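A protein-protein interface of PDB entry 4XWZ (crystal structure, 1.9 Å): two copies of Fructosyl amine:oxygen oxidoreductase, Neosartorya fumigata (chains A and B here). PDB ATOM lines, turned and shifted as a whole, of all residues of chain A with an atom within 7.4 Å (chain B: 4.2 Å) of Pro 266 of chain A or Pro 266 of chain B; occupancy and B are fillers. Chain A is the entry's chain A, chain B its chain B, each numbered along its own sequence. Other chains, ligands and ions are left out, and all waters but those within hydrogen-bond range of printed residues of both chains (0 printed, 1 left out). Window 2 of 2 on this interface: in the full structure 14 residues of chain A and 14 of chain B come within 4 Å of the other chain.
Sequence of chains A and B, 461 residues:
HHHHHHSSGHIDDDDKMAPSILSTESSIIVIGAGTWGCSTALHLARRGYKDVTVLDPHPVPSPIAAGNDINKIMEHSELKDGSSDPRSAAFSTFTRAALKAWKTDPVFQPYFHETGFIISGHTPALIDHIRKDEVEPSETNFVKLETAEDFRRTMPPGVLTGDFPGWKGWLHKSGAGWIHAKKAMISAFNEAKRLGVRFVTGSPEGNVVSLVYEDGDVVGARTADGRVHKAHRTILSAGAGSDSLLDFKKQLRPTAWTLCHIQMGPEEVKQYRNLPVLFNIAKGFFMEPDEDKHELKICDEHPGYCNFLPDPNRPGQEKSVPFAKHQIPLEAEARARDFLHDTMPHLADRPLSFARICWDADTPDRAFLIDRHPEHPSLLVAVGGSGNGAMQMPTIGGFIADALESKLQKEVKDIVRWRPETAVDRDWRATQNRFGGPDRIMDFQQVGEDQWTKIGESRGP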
ATOM      1  N   GLN A 263      13.378 -33.707   4.539  1.00  0.00           N
ATOM      2  CA  GLN A 263      13.546 -33.671   5.982  1.00  0.00           C
ATOM      3  C   GLN A 263      13.327 -32.256   6.516  1.00  0.00           C
ATOM      4  O   GLN A 263      13.958 -31.319   6.051  1.00  0.00           O
ATOM      5  CB  GLN A 263      14.955 -34.151   6.335  1.00  0.00           C
ATOM      6  CG  GLN A 263      15.389 -33.828   7.749  1.00  0.00           C
ATOM      7  CD  GLN A 263      14.811 -34.794   8.755  1.00  0.00           C
ATOM      8  OE1 GLN A 263      15.363 -35.871   8.981  1.00  0.00           O
ATOM      9  NE2 GLN A 263      13.620 -34.480   9.252  1.00  0.00           N
ATOM     10  N   MET A 264      12.283 -32.082   7.320  1.00  0.00           N
ATOM     11  CA  MET A 264      11.942 -30.768   7.851  1.00  0.00           C
ATOM     12  C   MET A 264      12.747 -30.475   9.108  1.00  0.00           C
ATOM     13  O   MET A 264      13.116 -31.385   9.850  1.00  0.00           O
ATOM     14  CB  MET A 264      10.445 -30.687   8.165  1.00  0.00           C
ATOM     15  CG  MET A 264       9.544 -31.080   7.005  1.00  0.00           C
ATOM     16  SD  MET A 264       9.721 -30.005   5.569  1.00  0.00           S
ATOM     17  CE  MET A 264       8.822 -28.560   6.131  1.00  0.00           C
ATOM     18  N   GLY A 265      13.026 -29.198   9.339  1.00  0.00           N
ATOM     19  CA  GLY A 265      13.757 -28.781  10.527  1.00  0.00           C
ATOM     20  C   GLY A 265      12.892 -28.749  11.769  1.00  0.00           C
ATOM     21  O   GLY A 265      11.663 -28.785  11.684  1.00  0.00           O
ATOM     22  N   PRO A 266      13.534 -28.640  12.942  1.00  0.00           N
ATOM     23  CA  PRO A 266      12.866 -28.889  14.216  1.00  0.00           C
ATOM     24  C   PRO A 266      11.913 -27.774  14.644  1.00  0.00           C
ATOM     25  O   PRO A 266      10.910 -28.047  15.303  1.00  0.00           O
ATOM     26  CB  PRO A 266      14.029 -29.025  15.210  1.00  0.00           C
ATOM     27  CG  PRO A 266      15.204 -28.394  14.539  1.00  0.00           C
ATOM     28  CD  PRO A 266      14.999 -28.633  13.075  1.00  0.00           C
ATOM     29  N   GLU A 267      12.130 -26.561  14.143  1.00  0.00           N
ATOM     30  CA  GLU A 267      11.197 -25.467  14.404  1.00  0.00           C
ATOM     31  C   GLU A 267      10.126 -25.383  13.322  1.00  0.00           C
ATOM     32  O   GLU A 267       8.937 -25.271  13.624  1.00  0.00           O
ATOM     33  CB  GLU A 267      11.934 -24.130  14.507  1.00  0.00           C
ATOM     34  CG  GLU A 267      12.789 -23.988  15.756  1.00  0.00           C
ATOM     35  CD  GLU A 267      12.014 -24.270  17.030  1.00  0.00           C
ATOM     36  OE1 GLU A 267      10.885 -23.754  17.166  1.00  0.00           O
ATOM     37  OE2 GLU A 267      12.481 -25.103  17.836  1.00  0.00           O
ATOM     38  N   GLU A 268      10.543 -25.445  12.061  1.00  0.00           N
ATOM     39  CA  GLU A 268       9.612 -25.229  10.960  1.00  0.00           C
ATOM     40  C   GLU A 268       8.551 -26.319  10.928  1.00  0.00           C
ATOM     41  O   GLU A 268       7.385 -26.042  10.648  1.00  0.00           O
ATOM     42  CB  GLU A 268      10.344 -25.153   9.617  1.00  0.00           C
ATOM     43  CG  GLU A 268      11.090 -26.417   9.243  1.00  0.00           C
ATOM     44  CD  GLU A 268      11.662 -26.370   7.841  1.00  0.00           C
ATOM     45  OE1 GLU A 268      11.407 -25.386   7.115  1.00  0.00           O
ATOM     46  OE2 GLU A 268      12.280 -27.371   7.430  1.00  0.00           O
ATOM     47  N   VAL A 269       8.910 -27.508  11.405  1.00  0.00           N
ATOM     48  CA  VAL A 269       8.008 -28.650  11.324  1.00  0.00           C
ATOM     49  C   VAL A 269       6.759 -28.449  12.177  1.00  0.00           C
ATOM     50  O   VAL A 269       5.732 -29.079  11.935  1.00  0.00           O
ATOM     51  CB  VAL A 269       8.697 -29.963  11.736  1.00  0.00           C
ATOM     52  CG1 VAL A 269       8.845 -30.046  13.245  1.00  0.00           C
ATOM     53  CG2 VAL A 269       7.909 -31.155  11.213  1.00  0.00           C
ATOM     54  N   LYS A 270       6.829 -27.542  13.145  1.00  0.00           N
ATOM     55  CA  LYS A 270       5.777 -27.437  14.147  1.00  0.00           C
ATOM     56  C   LYS A 270       4.517 -26.773  13.591  1.00  0.00           C
ATOM     57  O   LYS A 270       3.427 -26.966  14.125  1.00  0.00           O
ATOM     58  CB  LYS A 270       6.285 -26.675  15.375  1.00  0.00           C
ATOM     59  CG  LYS A 270       7.406 -27.390  16.119  1.00  0.00           C
ATOM     60  CD  LYS A 270       7.832 -26.628  17.367  1.00  0.00           C
ATOM     61  CE  LYS A 270       8.902 -27.383  18.141  1.00  0.00           C
ATOM     62  NZ  LYS A 270       9.772 -26.469  18.931  1.00  0.00           N
ATOM     63  N   GLN A 271       4.648 -26.076  12.467  1.00  0.00           N
ATOM     64  CA  GLN A 271       3.484 -25.505  11.793  1.00  0.00           C
ATOM     65  C   GLN A 271       2.744 -26.561  10.974  1.00  0.00           C
ATOM     66  O   GLN A 271       1.578 -26.369  10.622  1.00  0.00           O
ATOM     67  CB  GLN A 271       3.900 -24.349  10.880  1.00  0.00           C
ATOM     68  CG  GLN A 271       4.086 -23.013  11.581  1.00  0.00           C
ATOM     69  CD  GLN A 271       2.867 -22.580  12.372  1.00  0.00           C
ATOM     70  OE1 GLN A 271       2.803 -22.798  13.578  1.00  0.00           O
ATOM     71  NE2 GLN A 271       1.995 -21.804  11.740  1.00  0.00           N
ATOM     72  N   ARG A 273       1.096 -29.338  11.020  1.00  0.00           N
ATOM     73  CA  ARG A 273       0.401 -30.271  11.891  1.00  0.00           C
ATOM     74  C   ARG A 273      -1.070 -30.306  11.526  1.00  0.00           C
ATOM     75  O   ARG A 273      -1.672 -29.265  11.264  1.00  0.00           O
ATOM     76  CB  ARG A 273       0.554 -29.844  13.351  1.00  0.00           C
ATOM     77  CG  ARG A 273       1.828 -30.338  14.013  1.00  0.00           C
ATOM     78  CD  ARG A 273       1.899 -29.880  15.461  1.00  0.00           C
ATOM     79  NE  ARG A 273       3.218 -30.100  16.051  1.00  0.00           N
ATOM     80  CZ  ARG A 273       3.696 -29.420  17.089  1.00  0.00           C
ATOM     81  NH1 ARG A 273       3.000 -28.416  17.605  1.00  0.00           N
ATOM     82  NH2 ARG A 273       4.892 -29.712  17.579  1.00  0.00           N
ATOM     83  N   HIS A 294      10.324 -36.504  11.008  1.00  0.00           N
ATOM     84  CA  HIS A 294       9.951 -35.185  10.495  1.00  0.00           C
ATOM     85  C   HIS A 294      10.127 -35.090   8.983  1.00  0.00           C
ATOM     86  O   HIS A 294      10.461 -34.027   8.456  1.00  0.00           O
ATOM     87  CB  HIS A 294      10.779 -34.095  11.164  1.00  0.00           C
ATOM     88  CG  HIS A 294      10.482 -33.918  12.619  1.00  0.00           C
ATOM     89  ND1 HIS A 294      11.351 -33.283  13.482  1.00  0.00           N
ATOM     90  CD2 HIS A 294       9.459 -34.371  13.381  1.00  0.00           C
ATOM     91  CE1 HIS A 294      10.840 -33.293  14.700  1.00  0.00           C
ATOM     92  NE2 HIS A 294       9.688 -33.937  14.664  1.00  0.00           N
ATOM     93  N   GLY B 265      14.994 -21.422  13.784  1.00  0.00           N
ATOM     94  CA  GLY B 265      15.551 -22.764  13.647  1.00  0.00           C
ATOM     95  C   GLY B 265      16.460 -22.904  12.443  1.00  0.00           C
ATOM     96  O   GLY B 265      16.572 -21.984  11.628  1.00  0.00           O
ATOM     97  N   PRO B 266      17.211 -24.013  12.390  1.00  0.00           N
ATOM     98  CA  PRO B 266      18.360 -24.128  11.499  1.00  0.00           C
ATOM     99  C   PRO B 266      17.972 -24.260  10.032  1.00  0.00           C
ATOM    100  O   PRO B 266      18.730 -23.841   9.161  1.00  0.00           O
ATOM    101  CB  PRO B 266      19.069 -25.404  11.983  1.00  0.00           C
ATOM    102  CG  PRO B 266      18.085 -26.111  12.858  1.00  0.00           C
ATOM    103  CD  PRO B 266      17.230 -25.033  13.450  1.00  0.00           C
ATOM    104  N   GLU B 267      16.792 -24.812   9.760  1.00  0.00           N
ATOM    105  CA  GLU B 267      16.283 -24.853   8.394  1.00  0.00           C
ATOM    106  C   GLU B 267      15.500 -23.587   8.058  1.00  0.00           C
ATOM    107  O   GLU B 267      15.693 -22.995   6.996  1.00  0.00           O
ATOM    108  CB  GLU B 267      15.410 -26.088   8.175  1.00  0.00           C
ATOM    109  CG  GLU B 267      16.178 -27.399   8.226  1.00  0.00           C
ATOM    110  CD  GLU B 267      17.230 -27.504   7.135  1.00  0.00           C
ATOM    111  OE1 GLU B 267      17.051 -26.884   6.066  1.00  0.00           O
ATOM    112  OE2 GLU B 267      18.252 -28.183   7.358  1.00  0.00           O
ATOM    113  N   GLU B 268      14.560 -23.216   8.919  1.00  0.00           N
ATOM    114  CA  GLU B 268      13.619 -22.155   8.583  1.00  0.00           C
ATOM    115  C   GLU B 268      14.354 -20.834   8.356  1.00  0.00           C
ATOM    116  O   GLU B 268      13.979 -20.052   7.480  1.00  0.00           O
ATOM    117  CB  GLU B 268      12.554 -21.999   9.673  1.00  0.00           C
ATOM    118  CG  GLU B 268      13.107 -21.617  11.027  1.00  0.00           C
ATOM    119  CD  GLU B 268      12.028 -21.212  12.012  1.00  0.00           C
ATOM    120  OE1 GLU B 268      10.830 -21.227  11.648  1.00  0.00           O
ATOM    121  OE2 GLU B 268      12.383 -20.905  13.165  1.00  0.00           O
ATOM    122  N   VAL B 269      15.493 -20.665   9.022  1.00  0.00           N
ATOM    123  CA  VAL B 269      16.218 -19.401   8.965  1.00  0.00           C
ATOM    124  C   VAL B 269      16.780 -19.119   7.574  1.00  0.00           C
ATOM    125  O   VAL B 269      17.032 -17.967   7.228  1.00  0.00           O
ATOM    126  CB  VAL B 269      17.361 -19.348   9.999  1.00  0.00           C
ATOM    127  CG1 VAL B 269      18.504 -20.266   9.589  1.00  0.00           C
ATOM    128  CG2 VAL B 269      17.853 -17.917  10.167  1.00  0.00           C
ATOM    129  N   LYS B 270      16.853 -20.149   6.736  1.00  0.00           N
ATOM    130  CA  LYS B 270      17.566 -20.044   5.467  1.00  0.00           C
ATOM    131  C   LYS B 270      16.755 -19.291   4.417  1.00  0.00           C
ATOM    132  O   LYS B 270      17.309 -18.799   3.437  1.00  0.00           O
ATOM    133  CB  LYS B 270      17.933 -21.435   4.943  1.00  0.00           C
ATOM    134  CG  LYS B 270      18.958 -22.158   5.800  1.00  0.00           C
ATOM    135  CD  LYS B 270      19.230 -23.562   5.284  1.00  0.00           C
ATOM    136  CE  LYS B 270      20.287 -24.260   6.124  1.00  0.00           C
ATOM    137  NZ  LYS B 270      20.323 -25.725   5.870  1.00  0.00           N
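The side-chain amino group (NZ) of Lys 270 of chain A lies within salt-bridge range of the side-chain carboxylate (OE2) of Glu 267 of chain A (3.2 Å). The side-chain carboxylate (OE2) of Glu 268 of chain B is in hydrogen-bond range of the backbone NH (N) of Gly 265 of chain B (2.7 Å). N of Gly 265 of chain A sits at hydrogen-bond distance from OE2 of Glu 268 of chain A (2.7 Å). The side-chain carboxylate of Glu 267 of chain B lies within salt-bridge range of the side-chain amino group of Lys 270 of chain B, 3.5 Å away.
CG of Glu 267 of chain B touches CA of Gly 265 of chain A (3.6 Å). Pro 266 of chain A touches Pro 266 of chain B (CD to CG, 3.99 Å). CA of Gly 265 of chain B touches CG of Glu 267 of chain A, at 3.7 Å. Glu 267 of chain A touches Glu 268 of chain B. CB of Glu 267 of chain B touches OE2 of Glu 268 of chain A, at 3.5 Å. Glu 268 of chain B touches Glu 268 of chain A (CB to CB, 3.9 Å).
Of the printed residues of chain B, Gly 265 of chain A touches Glu 267. Of the printed residues of chain B, Pro 266 of chain A touches Pro 266 (3.99 Å). Of the printed residues of chain B, Glu 268 of chain A touches Glu 267 (3.5 Å) and Glu 268 (3.9 Å). Of the printed residues of chain A, Pro 266 of chain B touches Pro 266. Of the printed residues of chain A, Glu 268 of chain B touches Glu 267 and Glu 268.
Of the 11 printed residues of chain A, 4 touch a printed residue of chain B. Hydrophobic or aromatic side chains of chain A that line the printed part of chain B: Pro 266. Hydrophobic or aromatic side chains of chain B within 4 Å of the printed part of chain A: Pro 266. Among the printed residues, 6 pairs touch across the chains. Among the printed residues, no Asp or Glu carboxylate lies within 4 Å of a Lys or Arg side-chain nitrogen of the other chain.
Gly 265 of chain A touches Glu 267 of chain B, and with the chains exchanged Glu 267 of chain A touches Gly 265 of chain B. Pro 266 of chain A touches its own counterpart, Pro 266 of chain B. Glu 267 of chain A touches Glu 268 of chain B, and with the chains exchanged Glu 268 of chain A touches Glu 267 of chain B. Glu 268 of chain A touches its own counterpart, Glu 268 of chain B. Of the 6 pairs that touch across the chains among the printed residues, 6 have their exchanged pair printed and touching as well.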
